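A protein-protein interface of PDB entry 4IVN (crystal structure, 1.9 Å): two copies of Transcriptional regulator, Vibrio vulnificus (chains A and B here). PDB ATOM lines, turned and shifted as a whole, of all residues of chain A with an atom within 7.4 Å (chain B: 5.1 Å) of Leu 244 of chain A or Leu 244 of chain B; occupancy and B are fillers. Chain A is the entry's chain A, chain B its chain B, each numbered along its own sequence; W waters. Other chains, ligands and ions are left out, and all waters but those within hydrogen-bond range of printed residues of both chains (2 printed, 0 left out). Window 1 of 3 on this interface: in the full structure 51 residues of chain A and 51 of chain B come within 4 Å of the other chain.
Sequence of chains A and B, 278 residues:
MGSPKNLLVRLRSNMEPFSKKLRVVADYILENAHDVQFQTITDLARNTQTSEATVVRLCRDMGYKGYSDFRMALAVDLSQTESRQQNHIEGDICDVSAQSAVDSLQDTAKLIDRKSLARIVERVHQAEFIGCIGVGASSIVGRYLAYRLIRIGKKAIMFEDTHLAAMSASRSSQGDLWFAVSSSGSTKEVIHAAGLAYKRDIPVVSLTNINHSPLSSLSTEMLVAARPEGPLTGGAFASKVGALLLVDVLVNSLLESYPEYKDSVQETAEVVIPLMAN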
ATOM      1  N   LEU A 105      38.730  -8.466   8.819  1.00  0.00           N
ATOM      2  CA  LEU A 105      38.960  -7.300   7.964  1.00  0.00           C
ATOM      3  C   LEU A 105      40.377  -7.302   7.497  1.00  0.00           C
ATOM      4  O   LEU A 105      40.657  -7.123   6.328  1.00  0.00           O
ATOM      5  CB  LEU A 105      38.635  -6.017   8.726  1.00  0.00           C
ATOM      6  CG  LEU A 105      37.116  -5.777   8.903  1.00  0.00           C
ATOM      7  CD1 LEU A 105      36.939  -4.730   9.997  1.00  0.00           C
ATOM      8  CD2 LEU A 105      36.563  -5.238   7.587  1.00  0.00           C
ATOM      9  N   THR A 108      40.907 -10.147   4.999  1.00  0.00           N
ATOM     10  CA  THR A 108      40.264  -9.804   3.722  1.00  0.00           C
ATOM     11  C   THR A 108      41.064  -8.768   2.906  1.00  0.00           C
ATOM     12  O   THR A 108      41.316  -8.956   1.692  1.00  0.00           O
ATOM     13  CB  THR A 108      38.791  -9.330   3.947  1.00  0.00           C
ATOM     14  OG1 THR A 108      38.038 -10.413   4.514  1.00  0.00           O
ATOM     15  CG2 THR A 108      38.112  -8.931   2.648  1.00  0.00           C
ATOM     16  N   ALA A 137      21.680 -14.316   5.410  1.00  0.00           N
ATOM     17  CA  ALA A 137      22.600 -13.264   5.826  1.00  0.00           C
ATOM     18  C   ALA A 137      23.218 -12.539   4.641  1.00  0.00           C
ATOM     19  O   ALA A 137      23.661 -11.379   4.776  1.00  0.00           O
ATOM     20  CB  ALA A 137      23.722 -13.792   6.679  1.00  0.00           C
ATOM     21  N   ILE A 140      21.874  -9.109   3.587  1.00  0.00           N
ATOM     22  CA  ILE A 140      22.398  -7.880   4.304  1.00  0.00           C
ATOM     23  C   ILE A 140      23.505  -7.275   3.465  1.00  0.00           C
ATOM     24  O   ILE A 140      23.555  -6.041   3.273  1.00  0.00           O
ATOM     25  CB  ILE A 140      22.948  -8.271   5.729  1.00  0.00           C
ATOM     26  CG1 ILE A 140      21.790  -8.467   6.742  1.00  0.00           C
ATOM     27  CG2 ILE A 140      23.928  -7.238   6.310  1.00  0.00           C
ATOM     28  CD1 ILE A 140      20.732  -9.495   6.383  1.00  0.00           C
ATOM     29  N   VAL A 141      24.373  -8.147   2.931  1.00  0.00           N
ATOM     30  CA  VAL A 141      25.491  -7.676   2.085  1.00  0.00           C
ATOM     31  C   VAL A 141      25.040  -7.092   0.736  1.00  0.00           C
ATOM     32  O   VAL A 141      25.541  -5.998   0.364  1.00  0.00           O
ATOM     33  CB  VAL A 141      26.599  -8.787   1.884  1.00  0.00           C
ATOM     34  CG1 VAL A 141      27.742  -8.283   0.968  1.00  0.00           C
ATOM     35  CG2 VAL A 141      27.090  -9.191   3.278  1.00  0.00           C
ATOM     36  N   GLY A 142      24.121  -7.800   0.057  1.00  0.00           N
ATOM     37  CA  GLY A 142      23.549  -7.368  -1.207  1.00  0.00           C
ATOM     38  C   GLY A 142      22.758  -6.039  -1.036  1.00  0.00           C
ATOM     39  O   GLY A 142      22.865  -5.138  -1.841  1.00  0.00           O
ATOM     40  N   ARG A 143      22.011  -5.885   0.068  1.00  0.00           N
ATOM     41  CA  ARG A 143      21.363  -4.610   0.370  1.00  0.00           C
ATOM     42  C   ARG A 143      22.371  -3.509   0.575  1.00  0.00           C
ATOM     43  O   ARG A 143      22.121  -2.385   0.181  1.00  0.00           O
ATOM     44  CB  ARG A 143      20.516  -4.736   1.665  1.00  0.00           C
ATOM     45  CG  ARG A 143      19.175  -5.497   1.524  1.00  0.00           C
ATOM     46  CD  ARG A 143      18.224  -4.989   0.390  1.00  0.00           C
ATOM     47  NE  ARG A 143      17.038  -5.885   0.099  1.00  0.00           N
ATOM     48  CZ  ARG A 143      16.004  -5.616  -0.725  1.00  0.00           C
ATOM     49  NH1 ARG A 143      15.982  -4.485  -1.446  1.00  0.00           N
ATOM     50  NH2 ARG A 143      14.962  -6.488  -0.819  1.00  0.00           N
ATOM     51  N   TYR A 144      23.453  -3.783   1.266  1.00  0.00           N
ATOM     52  CA  TYR A 144      24.442  -2.693   1.424  1.00  0.00           C
ATOM     53  C   TYR A 144      25.015  -2.280   0.080  1.00  0.00           C
ATOM     54  O   TYR A 144      25.242  -1.112  -0.170  1.00  0.00           O
ATOM     55  CB  TYR A 144      25.568  -3.083   2.396  1.00  0.00           C
ATOM     56  CG  TYR A 144      26.467  -1.898   2.761  1.00  0.00           C
ATOM     57  CD1 TYR A 144      25.922  -0.680   3.351  1.00  0.00           C
ATOM     58  CD2 TYR A 144      27.864  -2.005   2.616  1.00  0.00           C
ATOM     59  CE1 TYR A 144      26.774   0.376   3.711  1.00  0.00           C
ATOM     60  CE2 TYR A 144      28.686  -0.958   2.991  1.00  0.00           C
ATOM     61  CZ  TYR A 144      28.124   0.215   3.531  1.00  0.00           C
ATOM     62  OH  TYR A 144      28.995   1.224   3.838  1.00  0.00           O
ATOM     63  N   LEU A 145      25.283  -3.256  -0.779  1.00  0.00           N
ATOM     64  CA  LEU A 145      25.758  -2.920  -2.141  1.00  0.00           C
ATOM     65  C   LEU A 145      24.754  -2.058  -2.953  1.00  0.00           C
ATOM     66  O   LEU A 145      25.169  -1.021  -3.553  1.00  0.00           O
ATOM     67  CB  LEU A 145      26.028  -4.260  -2.888  1.00  0.00           C
ATOM     68  CG  LEU A 145      26.541  -4.128  -4.359  1.00  0.00           C
ATOM     69  CD1 LEU A 145      27.822  -3.226  -4.427  1.00  0.00           C
ATOM     70  CD2 LEU A 145      26.868  -5.586  -4.777  1.00  0.00           C
ATOM     71  N   ARG A 148      24.846   1.376  -1.543  1.00  0.00           N
ATOM     72  CA  ARG A 148      25.994   2.168  -1.840  1.00  0.00           C
ATOM     73  C   ARG A 148      25.991   2.589  -3.383  1.00  0.00           C
ATOM     74  O   ARG A 148      26.429   3.710  -3.759  1.00  0.00           O
ATOM     75  CB  ARG A 148      27.313   1.387  -1.533  1.00  0.00           C
ATOM     76  CG  ARG A 148      27.585   1.213  -0.023  1.00  0.00           C
ATOM     77  CD  ARG A 148      27.781   2.597   0.642  1.00  0.00           C
ATOM     78  NE  ARG A 148      28.998   3.214   0.127  1.00  0.00           N
ATOM     79  CZ  ARG A 148      30.260   2.886   0.413  1.00  0.00           C
ATOM     80  NH1 ARG A 148      30.566   1.949   1.312  1.00  0.00           N
ATOM     81  NH2 ARG A 148      31.237   3.521  -0.235  1.00  0.00           N
ATOM     82  N   LEU A 207      30.399 -12.234  -4.993  1.00  0.00           N
ATOM     83  CA  LEU A 207      31.031 -11.816  -3.746  1.00  0.00           C
ATOM     84  C   LEU A 207      30.879 -12.910  -2.730  1.00  0.00           C
ATOM     85  O   LEU A 207      29.771 -13.114  -2.256  1.00  0.00           O
ATOM     86  CB  LEU A 207      30.353 -10.597  -3.203  1.00  0.00           C
ATOM     87  CG  LEU A 207      30.351  -9.315  -4.033  1.00  0.00           C
ATOM     88  CD1 LEU A 207      29.853  -8.149  -3.165  1.00  0.00           C
ATOM     89  CD2 LEU A 207      31.767  -8.969  -4.564  1.00  0.00           C
ATOM     90  N   ALA A 225      36.070 -12.750   0.279  1.00  0.00           N
ATOM     91  CA  ALA A 225      36.326 -12.268   1.670  1.00  0.00           C
ATOM     92  C   ALA A 225      36.870 -13.448   2.500  1.00  0.00           C
ATOM     93  O   ALA A 225      36.576 -14.624   2.165  1.00  0.00           O
ATOM     94  CB  ALA A 225      34.930 -11.788   2.247  1.00  0.00           C
ATOM     95  N   PHE A 237      29.486 -12.761  12.056  1.00  0.00           N
ATOM     96  CA  PHE A 237      29.833 -11.385  11.712  1.00  0.00           C
ATOM     97  C   PHE A 237      31.269 -11.333  11.124  1.00  0.00           C
ATOM     98  O   PHE A 237      31.543 -10.564  10.250  1.00  0.00           O
ATOM     99  CB  PHE A 237      29.671 -10.534  12.969  1.00  0.00           C
ATOM    100  CG  PHE A 237      30.078  -9.102  12.820  1.00  0.00           C
ATOM    101  CD1 PHE A 237      29.594  -8.292  11.778  1.00  0.00           C
ATOM    102  CD2 PHE A 237      31.005  -8.543  13.741  1.00  0.00           C
ATOM    103  CE1 PHE A 237      29.955  -6.941  11.692  1.00  0.00           C
ATOM    104  CE2 PHE A 237      31.343  -7.193  13.635  1.00  0.00           C
ATOM    105  CZ  PHE A 237      30.852  -6.411  12.632  1.00  0.00           C
ATOM    106  N   SER A 239      32.505 -13.377   9.020  1.00  0.00           N
ATOM    107  CA  SER A 239      32.363 -13.659   7.585  1.00  0.00           C
ATOM    108  C   SER A 239      31.695 -12.499   6.818  1.00  0.00           C
ATOM    109  O   SER A 239      32.147 -12.127   5.718  1.00  0.00           O
ATOM    110  CB  SER A 239      31.556 -14.914   7.367  1.00  0.00           C
ATOM    111  OG  SER A 239      32.309 -15.969   7.917  1.00  0.00           O
ATOM    112  N   LYS A 240      30.687 -11.895   7.410  1.00  0.00           N
ATOM    113  CA  LYS A 240      29.975 -10.834   6.741  1.00  0.00           C
ATOM    114  C   LYS A 240      30.792  -9.532   6.718  1.00  0.00           C
ATOM    115  O   LYS A 240      30.663  -8.735   5.800  1.00  0.00           O
ATOM    116  CB  LYS A 240      28.635 -10.563   7.442  1.00  0.00           C
ATOM    117  CG  LYS A 240      27.627 -11.747   7.446  1.00  0.00           C
ATOM    118  CD  LYS A 240      27.242 -12.269   6.018  1.00  0.00           C
ATOM    119  CE  LYS A 240      27.969 -13.554   5.652  1.00  0.00           C
ATOM    120  NZ  LYS A 240      27.394 -14.162   4.353  1.00  0.00           N
ATOM    121  N   VAL A 241      31.628  -9.321   7.724  1.00  0.00           N
ATOM    122  CA  VAL A 241      32.331  -8.058   7.795  1.00  0.00           C
ATOM    123  C   VAL A 241      33.302  -7.974   6.627  1.00  0.00           C
ATOM    124  O   VAL A 241      33.470  -6.918   6.026  1.00  0.00           O
ATOM    125  CB  VAL A 241      32.967  -7.795   9.180  1.00  0.00           C
ATOM    126  CG1 VAL A 241      34.280  -8.550   9.321  1.00  0.00           C
ATOM    127  CG2 VAL A 241      33.212  -6.285   9.341  1.00  0.00           C
ATOM    128  N   GLY A 242      33.919  -9.075   6.238  1.00  0.00           N
ATOM    129  CA  GLY A 242      34.802  -8.957   5.086  1.00  0.00           C
ATOM    130  C   GLY A 242      34.074  -8.796   3.766  1.00  0.00           C
ATOM    131  O   GLY A 242      34.601  -8.147   2.852  1.00  0.00           O
ATOM    132  N   ALA A 243      32.880  -9.419   3.662  1.00  0.00           N
ATOM    133  CA  ALA A 243      31.995  -9.272   2.431  1.00  0.00           C
ATOM    134  C   ALA A 243      31.585  -7.787   2.307  1.00  0.00           C
ATOM    135  O   ALA A 243      31.703  -7.169   1.219  1.00  0.00           O
ATOM    136  CB  ALA A 243      30.795 -10.203   2.481  1.00  0.00           C
ATOM    137  N   LEU A 244      31.257  -7.167   3.446  1.00  0.00           N
ATOM    138  CA  LEU A 244      30.953  -5.728   3.416  1.00  0.00           C
ATOM    139  C   LEU A 244      32.137  -4.839   3.081  1.00  0.00           C
ATOM    140  O   LEU A 244      31.948  -3.862   2.365  1.00  0.00           O
ATOM    141  CB  LEU A 244      30.310  -5.284   4.750  1.00  0.00           C
ATOM    142  CG  LEU A 244      28.979  -5.919   5.072  1.00  0.00           C
ATOM    143  CD1 LEU A 244      28.682  -5.746   6.623  1.00  0.00           C
ATOM    144  CD2 LEU A 244      27.798  -5.445   4.176  1.00  0.00           C
ATOM    145  N   LEU A 245      33.337  -5.126   3.627  1.00  0.00           N
ATOM    146  CA  LEU A 245      34.558  -4.445   3.207  1.00  0.00           C
ATOM    147  C   LEU A 245      34.786  -4.497   1.658  1.00  0.00           C
ATOM    148  O   LEU A 245      35.082  -3.483   1.043  1.00  0.00           O
ATOM    149  CB  LEU A 245      35.748  -5.076   3.889  1.00  0.00           C
ATOM    150  CG  LEU A 245      37.126  -4.539   3.465  1.00  0.00           C
ATOM    151  CD1 LEU A 245      37.288  -3.100   3.900  1.00  0.00           C
ATOM    152  CD2 LEU A 245      38.254  -5.384   4.065  1.00  0.00           C
ATOM    153  N   LEU A 246      34.627  -5.665   1.051  1.00  0.00           N
ATOM    154  CA  LEU A 246      34.619  -5.754  -0.445  1.00  0.00           C
ATOM    155  C   LEU A 246      33.670  -4.764  -1.094  1.00  0.00           C
ATOM    156  O   LEU A 246      34.063  -4.125  -2.102  1.00  0.00           O
ATOM    157  CB  LEU A 246      34.203  -7.150  -0.976  1.00  0.00           C
ATOM    158  CG  LEU A 246      34.915  -8.412  -0.493  1.00  0.00           C
ATOM    159  CD1 LEU A 246      34.243  -9.638  -1.153  1.00  0.00           C
ATOM    160  CD2 LEU A 246      36.424  -8.386  -0.686  1.00  0.00           C
ATOM    161  N   VAL A 247      32.429  -4.678  -0.589  1.00  0.00           N
ATOM    162  CA  VAL A 247      31.461  -3.674  -1.099  1.00  0.00           C
ATOM    163  C   VAL A 247      32.028  -2.260  -0.932  1.00  0.00           C
ATOM    164  O   VAL A 247      32.000  -1.384  -1.884  1.00  0.00           O
ATOM    165  CB  VAL A 247      30.060  -3.739  -0.423  1.00  0.00           C
ATOM    166  CG1 VAL A 247      29.220  -2.553  -0.828  1.00  0.00           C
ATOM    167  CG2 VAL A 247      29.257  -5.004  -0.814  1.00  0.00           C
ATOM    168  N   ASP A 248      32.576  -1.990   0.263  1.00  0.00           N
ATOM    169  CA  ASP A 248      33.079  -0.628   0.498  1.00  0.00           C
ATOM    170  C   ASP A 248      34.224  -0.247  -0.418  1.00  0.00           C
ATOM    171  O   ASP A 248      34.201   0.860  -0.993  1.00  0.00           O
ATOM    172  CB  ASP A 248      33.507  -0.478   1.969  1.00  0.00           C
ATOM    173  CG  ASP A 248      33.806   0.941   2.340  1.00  0.00           C
ATOM    174  OD1 ASP A 248      33.013   1.917   2.076  1.00  0.00           O
ATOM    175  OD2 ASP A 248      34.781   1.040   3.005  1.00  0.00           O
ATOM    176  N   VAL A 249      35.224  -1.147  -0.522  1.00  0.00           N
ATOM    177  CA  VAL A 249      36.361  -0.961  -1.413  1.00  0.00           C
ATOM    178  C   VAL A 249      35.934  -0.860  -2.877  1.00  0.00           C
ATOM    179  O   VAL A 249      36.408   0.014  -3.615  1.00  0.00           O
ATOM    180  CB  VAL A 249      37.401  -2.086  -1.199  1.00  0.00           C
ATOM    181  CG1 VAL A 249      38.534  -1.904  -2.161  1.00  0.00           C
ATOM    182  CG2 VAL A 249      37.925  -2.100   0.250  1.00  0.00           C
ATOM    183  N   LEU A 250      34.922  -1.620  -3.275  1.00  0.00           N
ATOM    184  CA  LEU A 250      34.442  -1.467  -4.625  1.00  0.00           C
ATOM    185  C   LEU A 250      33.992  -0.046  -4.855  1.00  0.00           C
ATOM    186  O   LEU A 250      34.384   0.553  -5.820  1.00  0.00           O
ATOM    187  CB  LEU A 250      33.318  -2.514  -4.937  1.00  0.00           C
ATOM    188  CG  LEU A 250      32.637  -2.404  -6.287  1.00  0.00           C
ATOM    189  CD1 LEU A 250      33.607  -2.426  -7.509  1.00  0.00           C
ATOM    190  CD2 LEU A 250      31.511  -3.463  -6.459  1.00  0.00           C
ATOM    191  N   ILE B 140      20.142  -2.054   6.520  1.00  0.00           N
ATOM    192  CA  ILE B 140      21.177  -3.170   6.491  1.00  0.00           C
ATOM    193  C   ILE B 140      21.437  -3.700   7.916  1.00  0.00           C
ATOM    194  O   ILE B 140      21.502  -4.922   8.143  1.00  0.00           O
ATOM    195  CB  ILE B 140      22.486  -2.683   5.822  1.00  0.00           C
ATOM    196  CG1 ILE B 140      22.323  -2.719   4.299  1.00  0.00           C
ATOM    197  CG2 ILE B 140      23.772  -3.404   6.339  1.00  0.00           C
ATOM    198  CD1 ILE B 140      21.389  -1.693   3.729  1.00  0.00           C
ATOM    199  N   VAL B 141      21.627  -2.767   8.857  1.00  0.00           N
ATOM    200  CA  VAL B 141      21.813  -3.096  10.241  1.00  0.00           C
ATOM    201  C   VAL B 141      20.598  -3.762  10.883  1.00  0.00           C
ATOM    202  O   VAL B 141      20.763  -4.772  11.579  1.00  0.00           O
ATOM    203  CB  VAL B 141      22.285  -1.859  11.029  1.00  0.00           C
ATOM    204  CG1 VAL B 141      22.426  -2.210  12.502  1.00  0.00           C
ATOM    205  CG2 VAL B 141      23.515  -1.298  10.309  1.00  0.00           C
ATOM    206  N   TYR B 144      20.270  -7.227   9.634  1.00  0.00           N
ATOM    207  CA  TYR B 144      21.199  -8.200  10.151  1.00  0.00           C
ATOM    208  C   TYR B 144      20.660  -8.603  11.545  1.00  0.00           C
ATOM    209  O   TYR B 144      20.810  -9.787  11.968  1.00  0.00           O
ATOM    210  CB  TYR B 144      22.637  -7.593  10.304  1.00  0.00           C
ATOM    211  CG  TYR B 144      23.631  -8.617  10.791  1.00  0.00           C
ATOM    212  CD1 TYR B 144      23.803  -9.807  10.075  1.00  0.00           C
ATOM    213  CD2 TYR B 144      24.489  -8.358  11.885  1.00  0.00           C
ATOM    214  CE1 TYR B 144      24.748 -10.740  10.456  1.00  0.00           C
ATOM    215  CE2 TYR B 144      25.440  -9.303  12.250  1.00  0.00           C
ATOM    216  CZ  TYR B 144      25.571 -10.450  11.555  1.00  0.00           C
ATOM    217  OH  TYR B 144      26.492 -11.377  11.996  1.00  0.00           O
ATOM    218  N   PHE B 237      30.978   2.954   5.758  1.00  0.00           N
ATOM    219  CA  PHE B 237      31.151   1.607   6.253  1.00  0.00           C
ATOM    220  C   PHE B 237      31.713   1.682   7.710  1.00  0.00           C
ATOM    221  O   PHE B 237      31.307   0.905   8.564  1.00  0.00           O
ATOM    222  CB  PHE B 237      32.109   0.854   5.315  1.00  0.00           C
ATOM    223  CG  PHE B 237      32.405  -0.554   5.767  1.00  0.00           C
ATOM    224  CD1 PHE B 237      31.363  -1.406   6.184  1.00  0.00           C
ATOM    225  CD2 PHE B 237      33.746  -1.033   5.815  1.00  0.00           C
ATOM    226  CE1 PHE B 237      31.628  -2.714   6.632  1.00  0.00           C
ATOM    227  CE2 PHE B 237      34.006  -2.370   6.227  1.00  0.00           C
ATOM    228  CZ  PHE B 237      32.951  -3.193   6.657  1.00  0.00           C
ATOM    229  N   LYS B 240      28.763   2.021   9.851  1.00  0.00           N
ATOM    230  CA  LYS B 240      27.822   0.873   9.866  1.00  0.00           C
ATOM    231  C   LYS B 240      28.457  -0.338  10.574  1.00  0.00           C
ATOM    232  O   LYS B 240      27.769  -1.198  11.161  1.00  0.00           O
ATOM    233  CB  LYS B 240      27.377   0.508   8.473  1.00  0.00           C
ATOM    234  CG  LYS B 240      26.544   1.501   7.640  1.00  0.00           C
ATOM    235  CD  LYS B 240      25.243   1.959   8.290  1.00  0.00           C
ATOM    236  CE  LYS B 240      25.509   3.178   9.160  1.00  0.00           C
ATOM    237  NZ  LYS B 240      24.189   3.622   9.674  1.00  0.00           N
ATOM    238  N   VAL B 241      29.779  -0.445  10.468  1.00  0.00           N
ATOM    239  CA  VAL B 241      30.511  -1.593  11.043  1.00  0.00           C
ATOM    240  C   VAL B 241      30.414  -1.619  12.565  1.00  0.00           C
ATOM    241  O   VAL B 241      30.215  -2.691  13.174  1.00  0.00           O
ATOM    242  CB  VAL B 241      31.998  -1.698  10.525  1.00  0.00           C
ATOM    243  CG1 VAL B 241      33.005  -0.775  11.254  1.00  0.00           C
ATOM    244  CG2 VAL B 241      32.483  -3.125  10.669  1.00  0.00           C
ATOM    245  N   GLY B 242      30.462  -0.432  13.173  1.00  0.00           N
ATOM    246  CA  GLY B 242      30.239  -0.401  14.619  1.00  0.00           C
ATOM    247  C   GLY B 242      28.838  -0.792  15.002  1.00  0.00           C
ATOM    248  O   GLY B 242      28.663  -1.468  16.020  1.00  0.00           O
ATOM    249  N   ALA B 243      27.839  -0.359  14.201  1.00  0.00           N
ATOM    250  CA  ALA B 243      26.454  -0.714  14.494  1.00  0.00           C
ATOM    251  C   ALA B 243      26.254  -2.204  14.358  1.00  0.00           C
ATOM    252  O   ALA B 243      25.576  -2.821  15.203  1.00  0.00           O
ATOM    253  CB  ALA B 243      25.484   0.025  13.544  1.00  0.00           C
ATOM    254  N   LEU B 244      26.807  -2.796  13.299  1.00  0.00           N
ATOM    255  CA  LEU B 244      26.788  -4.247  13.193  1.00  0.00           C
ATOM    256  C   LEU B 244      27.512  -4.912  14.335  1.00  0.00           C
ATOM    257  O   LEU B 244      27.078  -5.969  14.777  1.00  0.00           O
ATOM    258  CB  LEU B 244      27.413  -4.714  11.867  1.00  0.00           C
ATOM    259  CG  LEU B 244      26.490  -4.293  10.685  1.00  0.00           C
ATOM    260  CD1 LEU B 244      27.328  -4.443   9.403  1.00  0.00           C
ATOM    261  CD2 LEU B 244      25.178  -5.021  10.472  1.00  0.00           C
ATOM    262  N   LEU B 245      28.645  -4.376  14.773  1.00  0.00           N
ATOM    263  CA  LEU B 245      29.269  -4.948  15.962  1.00  0.00           C
ATOM    264  C   LEU B 245      28.318  -4.943  17.198  1.00  0.00           C
ATOM    265  O   LEU B 245      28.272  -5.956  17.904  1.00  0.00           O
ATOM    266  CB  LEU B 245      30.616  -4.249  16.318  1.00  0.00           C
ATOM    267  CG  LEU B 245      31.231  -4.771  17.617  1.00  0.00           C
ATOM    268  CD1 LEU B 245      31.702  -6.273  17.511  1.00  0.00           C
ATOM    269  CD2 LEU B 245      32.388  -3.872  17.997  1.00  0.00           C
ATOM    270  N   LEU B 246      27.553  -3.859  17.453  1.00  0.00           N
ATOM    271  CA  LEU B 246      26.542  -3.864  18.534  1.00  0.00           C
ATOM    272  C   LEU B 246      25.585  -5.087  18.428  1.00  0.00           C
ATOM    273  O   LEU B 246      25.270  -5.724  19.442  1.00  0.00           O
ATOM    274  CB  LEU B 246      25.718  -2.572  18.514  1.00  0.00           C
ATOM    275  CG  LEU B 246      26.547  -1.271  18.704  1.00  0.00           C
ATOM    276  CD1 LEU B 246      25.686  -0.018  18.766  1.00  0.00           C
ATOM    277  CD2 LEU B 246      27.430  -1.342  19.931  1.00  0.00           C
ATOM    278  N   VAL B 247      25.131  -5.394  17.200  1.00  0.00           N
ATOM    279  CA  VAL B 247      24.237  -6.514  16.968  1.00  0.00           C
ATOM    280  C   VAL B 247      24.917  -7.839  17.299  1.00  0.00           C
ATOM    281  O   VAL B 247      24.340  -8.669  18.054  1.00  0.00           O
ATOM    282  CB  VAL B 247      23.724  -6.513  15.490  1.00  0.00           C
ATOM    283  CG1 VAL B 247      23.014  -7.798  15.149  1.00  0.00           C
ATOM    284  CG2 VAL B 247      22.857  -5.307  15.193  1.00  0.00           C
ATOM    285  N   ASP B 248      26.141  -8.035  16.771  1.00  0.00           N
ATOM    286  CA  ASP B 248      26.917  -9.180  17.036  1.00  0.00           C
ATOM    287  C   ASP B 248      27.116  -9.415  18.538  1.00  0.00           C
ATOM    288  O   ASP B 248      26.889 -10.550  19.038  1.00  0.00           O
ATOM    289  CB  ASP B 248      28.270  -9.105  16.294  1.00  0.00           C
ATOM    290  CG  ASP B 248      29.013 -10.404  16.358  1.00  0.00           C
ATOM    291  OD1 ASP B 248      28.402 -11.457  16.081  1.00  0.00           O
ATOM    292  OD2 ASP B 248      30.211 -10.384  16.671  1.00  0.00           O
HETATM  293  O   HOH W   1      32.184   3.983   3.307  1.00  0.00           O
HETATM  294  O   HOH W   2      28.908 -13.612  14.682  1.00  0.00           O
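Among the printed residues, merely in contact across the chains: Leu 244 of chain A with Leu 244 of chain B, Phe 237 of chain A with Leu 244 of chain B, Tyr 144 of chain A with Ile 140 of chain B, Asp 248 of chain A with Phe 237 of chain B, Leu 244 of chain A with Phe 237 of chain B, Phe 237 of chain A with Asp 248 of chain B, Ile 140 of chain A with Tyr 144 of chain B, Val 241 of chain A with Val 241 of chain B, Leu 245 of chain A with Phe 237 of chain B, Phe 237 of chain A with Leu 245 of chain B, Arg 143 of chain A with Ile 140 of chain B, Ile 140 of chain A with Ile 140 of chain B, Phe 237 of chain A with Val 241 of chain B and Val 241 of chain A with Phe 237 of chain B.
Thr 108 of chain A touches none of the printed residues of chain B.
Printed residues of chain B within 4 Å of Val 241 of chain A: Phe 237 (3.8 Å) and Val 241 (3.5 Å).
Leu 244 of chain A touches two residues of chain B.
Of the printed residues of chain B, Leu 245 of chain A touches Phe 237 (3.6 Å).
Printed residues of chain B within 4 Å of Asp 248 of chain A: Phe 237.
No residue of chain A comes within 4 Å of Ala 243 of chain B.
Leu 246 of chain B touches none of the printed residues of chain A.
The nearest printed residue of chain A that does not touch Tyr 144 of chain B is Lys 240 of chain A (4.3 Å).
Water W1 lies within hydrogen-bond range of OD1 of Asp 248 of chain A (2.5 Å), N of Phe 237 of chain B (2.9 Å) and NH1 of Arg 148 of chain A (3.3 Å).
Water W2 bridges OD1 of Asp 248 of chain B (2.6 Å) and N of Phe 237 of chain A (2.8 Å).
Hydrophobic or aromatic side chains of chain B within 4 Å of the printed part of chain A: Ile 140, Tyr 144, Phe 237, Val 241, Leu 244 and Leu 245.
Of the 25 printed residues of chain A, 8 touch a printed residue of chain B.
Hydrophobic or aromatic side chains of chain A that line the printed part of chain B: Ile 140, Tyr 144, Phe 237, Val 241, Leu 244 and Leu 245.
OH of Tyr 144 of chain A is in hydrogen-bond range of NH1 of Arg 148 of chain A (3.1 Å).
The guanidinium group (NH1) of Arg 148 of chain A is in salt-bridge range of the side-chain carboxylate (OD1) of Asp 248 of chain A (2.6 Å).
Ile 140 of chain A touches its own counterpart, Ile 140 of chain B.
Phe 237 of chain A touches Leu 244 of chain B, and with the chains exchanged Leu 244 of chain A touches Phe 237 of chain B.
Phe 237 of chain A touches Leu 245 of chain B, and with the chains exchanged Leu 245 of chain A touches Phe 237 of chain B.
Phe 237 of chain A touches Asp 248 of chain B, and with the chains exchanged Asp 248 of chain A touches Phe 237 of chain B.
Of the 16 pairs that touch across the chains among the printed residues, 15 have their exchanged pair printed and touching as well.
The side-chain hydroxyl (OH) of Tyr 144 of chain A sits at hydrogen-bond distance from the backbone NH (N) of Phe 237 of chain B (3.3 Å).
The backbone NH (N) of Phe 237 of chain A sits at hydrogen-bond distance from the side-chain hydroxyl (OH) of Tyr 144 of chain B (3.3 Å).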
